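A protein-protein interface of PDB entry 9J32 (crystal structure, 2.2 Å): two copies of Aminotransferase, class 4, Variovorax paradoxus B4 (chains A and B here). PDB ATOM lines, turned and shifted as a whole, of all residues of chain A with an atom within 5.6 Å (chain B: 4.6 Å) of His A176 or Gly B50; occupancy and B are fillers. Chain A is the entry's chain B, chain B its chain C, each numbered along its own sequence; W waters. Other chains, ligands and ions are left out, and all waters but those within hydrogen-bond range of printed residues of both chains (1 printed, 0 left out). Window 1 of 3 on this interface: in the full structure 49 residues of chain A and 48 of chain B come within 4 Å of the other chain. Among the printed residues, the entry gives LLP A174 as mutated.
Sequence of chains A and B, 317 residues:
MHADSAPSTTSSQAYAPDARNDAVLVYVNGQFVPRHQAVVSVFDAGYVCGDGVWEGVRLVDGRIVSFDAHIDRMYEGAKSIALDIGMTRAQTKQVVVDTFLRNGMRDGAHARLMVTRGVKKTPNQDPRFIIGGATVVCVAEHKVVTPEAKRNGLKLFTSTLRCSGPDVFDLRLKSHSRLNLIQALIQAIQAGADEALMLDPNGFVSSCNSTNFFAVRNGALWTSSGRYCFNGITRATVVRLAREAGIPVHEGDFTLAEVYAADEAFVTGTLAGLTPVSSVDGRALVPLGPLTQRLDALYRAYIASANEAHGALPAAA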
ATOM      1  N   GLY A  46     -26.886 -11.458  20.312  1.00  0.00           N
ATOM      2  CA  GLY A  46     -26.063 -12.646  20.172  1.00  0.00           C
ATOM      3  C   GLY A  46     -26.857 -13.881  19.718  1.00  0.00           C
ATOM      4  O   GLY A  46     -26.449 -14.607  18.802  1.00  0.00           O
ATOM      5  N   CYS A  49     -29.093 -12.884  16.174  1.00  0.00           N
ATOM      6  CA  CYS A  49     -28.448 -12.363  14.978  1.00  0.00           C
ATOM      7  C   CYS A  49     -26.998 -12.880  14.890  1.00  0.00           C
ATOM      8  O   CYS A  49     -26.346 -12.773  13.850  1.00  0.00           O
ATOM      9  CB  CYS A  49     -28.516 -10.824  15.015  1.00  0.00           C
ATOM     10  SG  CYS A  49     -30.012 -10.029  14.333  1.00  0.00           S
ATOM     11  N   GLY A  50     -26.454 -13.528  15.929  1.00  0.00           N
ATOM     12  CA  GLY A  50     -25.045 -13.890  15.942  1.00  0.00           C
ATOM     13  C   GLY A  50     -24.138 -12.676  16.120  1.00  0.00           C
ATOM     14  O   GLY A  50     -22.979 -12.737  15.759  1.00  0.00           O
ATOM     15  N   ASP A  51     -24.661 -11.608  16.742  1.00  0.00           N
ATOM     16  CA  ASP A  51     -24.118 -10.262  16.627  1.00  0.00           C
ATOM     17  C   ASP A  51     -23.285  -9.916  17.887  1.00  0.00           C
ATOM     18  O   ASP A  51     -23.814  -9.423  18.881  1.00  0.00           O
ATOM     19  CB  ASP A  51     -25.240  -9.317  16.217  1.00  0.00           C
ATOM     20  CG  ASP A  51     -24.828  -7.842  16.223  1.00  0.00           C
ATOM     21  OD1 ASP A  51     -23.613  -7.545  16.328  1.00  0.00           O
ATOM     22  OD2 ASP A  51     -25.706  -6.984  16.136  1.00  0.00           O
ATOM     23  N   GLY A  52     -21.999 -10.295  17.854  1.00  0.00           N
ATOM     24  CA  GLY A  52     -21.033 -10.053  18.902  1.00  0.00           C
ATOM     25  C   GLY A  52     -19.668 -10.601  18.523  1.00  0.00           C
ATOM     26  O   GLY A  52     -19.525 -11.276  17.508  1.00  0.00           O
ATOM     27  N   VAL A  53     -18.680 -10.305  19.372  1.00  0.00           N
ATOM     28  CA  VAL A  53     -17.320 -10.796  19.278  1.00  0.00           C
ATOM     29  C   VAL A  53     -16.928 -11.526  20.551  1.00  0.00           C
ATOM     30  O   VAL A  53     -17.454 -11.261  21.631  1.00  0.00           O
ATOM     31  CB  VAL A  53     -16.343  -9.656  18.956  1.00  0.00           C
ATOM     32  CG1 VAL A  53     -16.634  -9.045  17.586  1.00  0.00           C
ATOM     33  CG2 VAL A  53     -16.375  -8.566  19.999  1.00  0.00           C
ATOM     34  N   TRP A  54     -15.973 -12.435  20.421  1.00  0.00           N
ATOM     35  CA  TRP A  54     -15.514 -13.199  21.562  1.00  0.00           C
ATOM     36  C   TRP A  54     -14.005 -13.455  21.546  1.00  0.00           C
ATOM     37  O   TRP A  54     -13.301 -13.147  20.574  1.00  0.00           O
ATOM     38  CB  TRP A  54     -16.312 -14.488  21.644  1.00  0.00           C
ATOM     39  CG  TRP A  54     -16.053 -15.452  20.528  1.00  0.00           C
ATOM     40  CD1 TRP A  54     -16.549 -15.417  19.263  1.00  0.00           C
ATOM     41  CD2 TRP A  54     -15.218 -16.616  20.611  1.00  0.00           C
ATOM     42  NE1 TRP A  54     -16.047 -16.461  18.530  1.00  0.00           N
ATOM     43  CE2 TRP A  54     -15.260 -17.235  19.339  1.00  0.00           C
ATOM     44  CE3 TRP A  54     -14.442 -17.180  21.619  1.00  0.00           C
ATOM     45  CZ2 TRP A  54     -14.553 -18.404  19.064  1.00  0.00           C
ATOM     46  CZ3 TRP A  54     -13.757 -18.338  21.356  1.00  0.00           C
ATOM     47  CH2 TRP A  54     -13.832 -18.957  20.099  1.00  0.00           C
ATOM     48  N   LEU A 113     -14.755 -15.178  26.607  1.00  0.00           N
ATOM     49  CA  LEU A 113     -15.325 -13.868  26.908  1.00  0.00           C
ATOM     50  C   LEU A 113     -16.182 -13.490  25.706  1.00  0.00           C
ATOM     51  O   LEU A 113     -15.676 -13.343  24.603  1.00  0.00           O
ATOM     52  CB  LEU A 113     -14.292 -12.785  27.252  1.00  0.00           C
ATOM     53  CG  LEU A 113     -14.785 -11.340  27.390  1.00  0.00           C
ATOM     54  CD1 LEU A 113     -15.727 -11.250  28.555  1.00  0.00           C
ATOM     55  CD2 LEU A 113     -13.588 -10.353  27.512  1.00  0.00           C
ATOM     56  N   MET A 114     -17.481 -13.329  25.932  1.00  0.00           N
ATOM     57  CA  MET A 114     -18.447 -13.065  24.883  1.00  0.00           C
ATOM     58  C   MET A 114     -19.082 -11.709  25.168  1.00  0.00           C
ATOM     59  O   MET A 114     -19.535 -11.435  26.290  1.00  0.00           O
ATOM     60  CB  MET A 114     -19.435 -14.220  24.844  1.00  0.00           C
ATOM     61  CG  MET A 114     -18.734 -15.543  24.484  1.00  0.00           C
ATOM     62  SD  MET A 114     -19.757 -17.009  24.488  1.00  0.00           S
ATOM     63  CE  MET A 114     -20.182 -17.061  26.240  1.00  0.00           C
ATOM     64  N   VAL A 115     -18.991 -10.831  24.173  1.00  0.00           N
ATOM     65  CA  VAL A 115     -19.618  -9.538  24.217  1.00  0.00           C
ATOM     66  C   VAL A 115     -20.526  -9.419  23.001  1.00  0.00           C
ATOM     67  O   VAL A 115     -20.029  -9.295  21.847  1.00  0.00           O
ATOM     68  CB  VAL A 115     -18.519  -8.466  24.228  1.00  0.00           C
ATOM     69  CG1 VAL A 115     -19.119  -7.078  24.303  1.00  0.00           C
ATOM     70  CG2 VAL A 115     -17.525  -8.678  25.360  1.00  0.00           C
ATOM     71  N   THR A 116     -21.838  -9.458  23.252  1.00  0.00           N
ATOM     72  CA  THR A 116     -22.840  -9.365  22.196  1.00  0.00           C
ATOM     73  C   THR A 116     -23.468  -7.985  22.251  1.00  0.00           C
ATOM     74  O   THR A 116     -23.293  -7.252  23.222  1.00  0.00           O
ATOM     75  CB  THR A 116     -23.832 -10.512  22.321  1.00  0.00           C
ATOM     76  OG1 THR A 116     -24.483 -10.589  23.591  1.00  0.00           O
ATOM     77  CG2 THR A 116     -23.153 -11.838  21.992  1.00  0.00           C
ATOM     78  N1  LLP A 174      -9.499 -20.093  13.930  1.00  0.00           N
ATOM     79  C2  LLP A 174     -10.673 -19.559  14.190  1.00  0.00           C
ATOM     80  C2' LLP A 174     -11.761 -19.665  13.163  1.00  0.00           C
ATOM     81  C3  LLP A 174     -10.879 -18.950  15.467  1.00  0.00           C
ATOM     82  O3  LLP A 174     -12.119 -18.449  15.781  1.00  0.00           O
ATOM     83  C4  LLP A 174      -9.859 -18.991  16.449  1.00  0.00           C
ATOM     84  C4' LLP A 174     -10.069 -18.326  17.715  1.00  0.00           C
ATOM     85  C5  LLP A 174      -8.613 -19.543  16.093  1.00  0.00           C
ATOM     86  C6  LLP A 174      -8.479 -20.049  14.826  1.00  0.00           C
ATOM     87  C5' LLP A 174      -7.458 -19.623  17.050  1.00  0.00           C
ATOM     88  OP4 LLP A 174      -7.010 -18.309  17.461  1.00  0.00           O
ATOM     89  P   LLP A 174      -5.975 -18.194  18.684  1.00  0.00           P
ATOM     90  OP1 LLP A 174      -6.729 -18.917  19.838  1.00  0.00           O
ATOM     91  OP2 LLP A 174      -4.726 -18.887  18.308  1.00  0.00           O
ATOM     92  OP3 LLP A 174      -5.829 -16.726  18.759  1.00  0.00           O
ATOM     93  N   LLP A 174     -13.555 -12.472  15.219  1.00  0.00           N
ATOM     94  CA  LLP A 174     -13.857 -13.618  16.065  1.00  0.00           C
ATOM     95  CB  LLP A 174     -12.833 -13.750  17.190  1.00  0.00           C
ATOM     96  CG  LLP A 174     -12.803 -15.073  17.921  1.00  0.00           C
ATOM     97  CD  LLP A 174     -11.513 -15.257  18.731  1.00  0.00           C
ATOM     98  CE  LLP A 174     -11.170 -16.705  19.074  1.00  0.00           C
ATOM     99  NZ  LLP A 174     -11.053 -17.552  17.886  1.00  0.00           N
ATOM    100  C   LLP A 174     -15.259 -13.341  16.563  1.00  0.00           C
ATOM    101  O   LLP A 174     -15.430 -12.594  17.537  1.00  0.00           O
ATOM    102  N   SER A 175     -16.259 -13.851  15.815  1.00  0.00           N
ATOM    103  CA  SER A 175     -17.634 -13.404  15.978  1.00  0.00           C
ATOM    104  C   SER A 175     -18.565 -14.524  16.440  1.00  0.00           C
ATOM    105  O   SER A 175     -18.187 -15.683  16.437  1.00  0.00           O
ATOM    106  CB  SER A 175     -18.121 -12.724  14.728  1.00  0.00           C
ATOM    107  OG  SER A 175     -18.851 -13.565  13.869  1.00  0.00           O
ATOM    108  N   HIS A 176     -19.802 -14.128  16.777  1.00  0.00           N
ATOM    109  CA  HIS A 176     -20.893 -15.024  17.163  1.00  0.00           C
ATOM    110  C   HIS A 176     -21.682 -15.533  15.948  1.00  0.00           C
ATOM    111  O   HIS A 176     -22.742 -16.099  16.111  1.00  0.00           O
ATOM    112  CB  HIS A 176     -21.761 -14.314  18.234  1.00  0.00           C
ATOM    113  CG  HIS A 176     -21.179 -14.389  19.611  1.00  0.00           C
ATOM    114  ND1 HIS A 176     -21.805 -15.062  20.642  1.00  0.00           N
ATOM    115  CD2 HIS A 176     -20.048 -13.857  20.130  1.00  0.00           C
ATOM    116  CE1 HIS A 176     -21.073 -14.924  21.748  1.00  0.00           C
ATOM    117  NE2 HIS A 176     -19.986 -14.234  21.451  1.00  0.00           N
ATOM    118  N   SER A 177     -21.219 -15.250  14.725  1.00  0.00           N
ATOM    119  CA  SER A 177     -21.843 -15.697  13.497  1.00  0.00           C
ATOM    120  C   SER A 177     -20.975 -16.785  12.868  1.00  0.00           C
ATOM    121  O   SER A 177     -20.146 -16.454  12.038  1.00  0.00           O
ATOM    122  CB  SER A 177     -21.984 -14.507  12.562  1.00  0.00           C
ATOM    123  OG  SER A 177     -23.088 -13.666  12.876  1.00  0.00           O
ATOM    124  N   ARG A 178     -21.163 -18.066  13.217  1.00  0.00           N
ATOM    125  CA  ARG A 178     -20.162 -19.086  12.941  1.00  0.00           C
ATOM    126  C   ARG A 178     -20.645 -20.215  12.040  1.00  0.00           C
ATOM    127  O   ARG A 178     -19.895 -21.163  11.839  1.00  0.00           O
ATOM    128  CB  ARG A 178     -19.591 -19.592  14.269  1.00  0.00           C
ATOM    129  CG  ARG A 178     -18.680 -18.527  14.864  1.00  0.00           C
ATOM    130  CD  ARG A 178     -17.995 -18.997  16.157  1.00  0.00           C
ATOM    131  NE  ARG A 178     -16.658 -19.488  15.814  1.00  0.00           N
ATOM    132  CZ  ARG A 178     -15.606 -18.741  15.457  1.00  0.00           C
ATOM    133  NH1 ARG A 178     -15.723 -17.449  15.199  1.00  0.00           N
ATOM    134  NH2 ARG A 178     -14.439 -19.304  15.254  1.00  0.00           N
ATOM    135  N   LEU A 179     -21.811 -20.073  11.395  1.00  0.00           N
ATOM    136  CA  LEU A 179     -22.355 -21.153  10.603  1.00  0.00           C
ATOM    137  C   LEU A 179     -21.504 -21.302   9.348  1.00  0.00           C
ATOM    138  O   LEU A 179     -21.478 -22.398   8.809  1.00  0.00           O
ATOM    139  CB  LEU A 179     -23.831 -20.914  10.259  1.00  0.00           C
ATOM    140  CG  LEU A 179     -24.838 -21.511  11.228  1.00  0.00           C
ATOM    141  CD1 LEU A 179     -26.171 -20.885  10.989  1.00  0.00           C
ATOM    142  CD2 LEU A 179     -24.926 -22.985  11.031  1.00  0.00           C
ATOM    143  N   ALA B  45     -26.088 -23.153  21.326  1.00  0.00           N
ATOM    144  CA  ALA B  45     -25.434 -22.931  20.024  1.00  0.00           C
ATOM    145  C   ALA B  45     -25.904 -21.653  19.306  1.00  0.00           C
ATOM    146  O   ALA B  45     -25.168 -21.065  18.513  1.00  0.00           O
ATOM    147  CB  ALA B  45     -25.701 -24.137  19.148  1.00  0.00           C
ATOM    148  N   GLY B  46     -27.137 -21.213  19.588  1.00  0.00           N
ATOM    149  CA  GLY B  46     -27.649 -19.994  19.001  1.00  0.00           C
ATOM    150  C   GLY B  46     -26.880 -18.756  19.448  1.00  0.00           C
ATOM    151  O   GLY B  46     -26.506 -17.928  18.613  1.00  0.00           O
ATOM    152  N   TYR B  47     -26.764 -18.600  20.770  1.00  0.00           N
ATOM    153  CA  TYR B  47     -26.049 -17.494  21.401  1.00  0.00           C
ATOM    154  C   TYR B  47     -24.552 -17.568  21.066  1.00  0.00           C
ATOM    155  O   TYR B  47     -23.929 -16.560  20.760  1.00  0.00           O
ATOM    156  CB  TYR B  47     -26.341 -17.462  22.913  1.00  0.00           C
ATOM    157  CG  TYR B  47     -25.448 -16.498  23.663  1.00  0.00           C
ATOM    158  CD1 TYR B  47     -25.667 -15.133  23.629  1.00  0.00           C
ATOM    159  CD2 TYR B  47     -24.332 -16.940  24.354  1.00  0.00           C
ATOM    160  CE1 TYR B  47     -24.832 -14.237  24.294  1.00  0.00           C
ATOM    161  CE2 TYR B  47     -23.451 -16.051  24.961  1.00  0.00           C
ATOM    162  CZ  TYR B  47     -23.701 -14.688  24.950  1.00  0.00           C
ATOM    163  OH  TYR B  47     -22.846 -13.793  25.558  1.00  0.00           O
ATOM    164  N   VAL B  48     -23.968 -18.754  21.135  1.00  0.00           N
ATOM    165  CA  VAL B  48     -22.518 -18.903  21.040  1.00  0.00           C
ATOM    166  C   VAL B  48     -22.018 -18.780  19.591  1.00  0.00           C
ATOM    167  O   VAL B  48     -20.953 -18.183  19.340  1.00  0.00           O
ATOM    168  CB  VAL B  48     -22.105 -20.245  21.687  1.00  0.00           C
ATOM    169  CG1 VAL B  48     -20.603 -20.478  21.652  1.00  0.00           C
ATOM    170  CG2 VAL B  48     -22.552 -20.330  23.166  1.00  0.00           C
ATOM    171  N   CYS B  49     -22.715 -19.481  18.690  1.00  0.00           N
ATOM    172  CA  CYS B  49     -22.219 -19.846  17.356  1.00  0.00           C
ATOM    173  C   CYS B  49     -23.117 -19.237  16.265  1.00  0.00           C
ATOM    174  O   CYS B  49     -22.774 -19.268  15.083  1.00  0.00           O
ATOM    175  CB  CYS B  49     -22.162 -21.372  17.233  1.00  0.00           C
ATOM    176  SG  CYS B  49     -20.716 -22.217  17.890  1.00  0.00           S
ATOM    177  N   GLY B  50     -24.264 -18.635  16.625  1.00  0.00           N
ATOM    178  CA  GLY B  50     -25.243 -18.203  15.632  1.00  0.00           C
ATOM    179  C   GLY B  50     -25.911 -19.377  14.914  1.00  0.00           C
ATOM    180  O   GLY B  50     -26.371 -19.214  13.799  1.00  0.00           O
ATOM    181  N   ASP B  51     -25.993 -20.533  15.589  1.00  0.00           N
ATOM    182  CA  ASP B  51     -26.229 -21.833  14.981  1.00  0.00           C
ATOM    183  C   ASP B  51     -27.703 -22.246  15.182  1.00  0.00           C
ATOM    184  O   ASP B  51     -28.061 -22.942  16.154  1.00  0.00           O
ATOM    185  CB  ASP B  51     -25.129 -22.788  15.428  1.00  0.00           C
ATOM    186  CG  ASP B  51     -25.333 -24.225  14.992  1.00  0.00           C
ATOM    187  OD1 ASP B  51     -26.241 -24.460  14.133  1.00  0.00           O
ATOM    188  OD2 ASP B  51     -24.631 -25.120  15.530  1.00  0.00           O
ATOM    189  N   GLY B  52     -28.549 -21.755  14.275  1.00  0.00           N
ATOM    190  CA  GLY B  52     -29.952 -22.098  14.173  1.00  0.00           C
ATOM    191  C   GLY B  52     -30.591 -21.508  12.920  1.00  0.00           C
ATOM    192  O   GLY B  52     -29.959 -20.764  12.179  1.00  0.00           O
ATOM    193  N   HIS B 176     -29.333 -17.829  12.227  1.00  0.00           N
ATOM    194  CA  HIS B 176     -28.938 -17.046  13.388  1.00  0.00           C
ATOM    195  C   HIS B 176     -27.538 -16.437  13.240  1.00  0.00           C
ATOM    196  O   HIS B 176     -27.014 -15.871  14.194  1.00  0.00           O
ATOM    197  CB  HIS B 176     -29.127 -17.909  14.654  1.00  0.00           C
ATOM    198  CG  HIS B 176     -30.547 -17.963  15.122  1.00  0.00           C
ATOM    199  ND1 HIS B 176     -30.941 -17.393  16.305  1.00  0.00           N
ATOM    200  CD2 HIS B 176     -31.658 -18.466  14.571  1.00  0.00           C
ATOM    201  CE1 HIS B 176     -32.239 -17.569  16.450  1.00  0.00           C
ATOM    202  NE2 HIS B 176     -32.710 -18.223  15.413  1.00  0.00           N
ATOM    203  N   SER B 177     -26.923 -16.560  12.056  1.00  0.00           N
ATOM    204  CA  SER B 177     -25.635 -15.962  11.767  1.00  0.00           C
ATOM    205  C   SER B 177     -25.837 -14.769  10.823  1.00  0.00           C
ATOM    206  O   SER B 177     -25.795 -14.937   9.633  1.00  0.00           O
ATOM    207  CB  SER B 177     -24.736 -17.028  11.155  1.00  0.00           C
ATOM    208  OG  SER B 177     -24.181 -17.885  12.135  1.00  0.00           O
HETATM  209  O   HOH W   1     -18.835 -17.130  21.048  1.00  0.00           O
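Printed residues of chain B within 4 Å of Gly A46: Gly B46 and Tyr B47. Printed residues of chain B within 4 Å of Thr A116: Tyr B47 (3.7 Å). Of chain B, only Tyr B47, Val B48, Cys B49 and Gly B50 come within 4 Å of His A176. Printed residues of chain B within 4 Å of Ser A177: Cys B49 and Ser B177. Of the printed residues of chain A, Val B48 touches His A176 (3.5 Å). Of chain A, only His A176 (3.0 Å) and Leu A179 (3.3 Å) come within 4 Å of Gly B50. The nearest residue of chain A that does not touch Gly B50 is Gly A50 (4.3 Å). The nearest printed residue of chain B that does not touch Ser A177 is His B176 (4.7 Å).
Water W1 lies within hydrogen-bond range of O of Val B48 (2.9 Å), NE2 of His A176 (3.1 Å) and SD of Met A114 (3.6 Å).
Cys A49 touches His B176, and with the chains exchanged His A176 touches Cys B49. Cys A49 touches Ser B177, and with the chains exchanged Ser A177 touches Cys B49. Gly A50 touches His B176, and with the chains exchanged His A176 touches Gly B50. Ser A177 touches its own counterpart, Ser B177. 7 positions are printed for both chains. Of the 20 pairs that touch across the chains among the printed residues, 8 have their exchanged pair printed and touching as well.
Hydrophobic or aromatic side chains of chain A that line the printed part of chain B: Met A114, His A176 and Leu A179. Of the 10 printed residues of chain B, 9 touch a printed residue of chain A. Among the printed residues, 20 pairs touch across the chains. Among the printed residues, no Asp or Glu carboxylate lies within 4 Å of a Lys or Arg side-chain nitrogen of the other chain.
The backbone NH (N) of Gly A50 lies within hydrogen-bond range of the backbone carbonyl oxygen (O) of His B176 (3.0 Å). A ring nitrogen (ND1) of His A176 is in hydrogen-bond range of the backbone carbonyl oxygen (O) of Tyr B47, 2.6 Å away. A ring nitrogen (ND1) of His A176 sits at hydrogen-bond distance from the backbone carbonyl oxygen (O) of Val B48. The backbone carbonyl oxygen of His A176 is in hydrogen-bond range of the backbone NH of Gly B50 (3.0 Å). The backbone carbonyl oxygen of Cys B49 sits at hydrogen-bond distance from the backbone NH of Arg A178 (2.7 Å). N of Arg A178 sits at hydrogen-bond distance from OG of Ser B177 (3.2 Å). The side-chain hydroxyl of Ser B177 lies within hydrogen-bond range of the backbone NH of Leu A179. The backbone carbonyl oxygen (O) of Gly B46 sits close to the backbone carbonyl oxygen (O) of Gly A46 (3.3 Å). O of His B176 lies close to O of Cys A49 (3.2 Å). O of His A176 sits close to O of Cys B49 (3.3 Å).
OG of Ser A177 is in hydrogen-bond range of O of Gly A50, 3.0 Å away. O of Gly A52 sits at hydrogen-bond distance from N of His A176 (3.0 Å). O3 of LLP A174 is in hydrogen-bond range of the guanidinium group of Arg A178, 2.5 Å away. OG of Ser A175 sits at hydrogen-bond distance from N of Ser A177, at 3.0 Å. O of Ala B45 lies within hydrogen-bond range of N of Asp B51, at 3.1 Å. The backbone carbonyl oxygen (O) of Gly B50 sits at hydrogen-bond distance from the side-chain hydroxyl (OG) of Ser B177 (3.1 Å).
Tyr B47 touches Gly A46. Ser B177 touches Cys A49 (C to O, 3.7 Å). OH of Tyr B47 touches CB of Met A114 (3.5 Å). CG2 of Thr A116 touches CE1 of Tyr B47, at 3.7 Å. C of Ser A177 touches O of Cys B49 (3.8 Å). Ser B177 touches Ser A177. O of Cys B49 touches N of Leu A179 (3.9 Å). O of Gly B50 touches CD1 of Leu A179 (3.3 Å). CD2 of Leu A179 touches OD1 of Asp B51 (3.7 Å). CD1 of Leu A179 touches O of Gly B52, 3.97 Å away.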
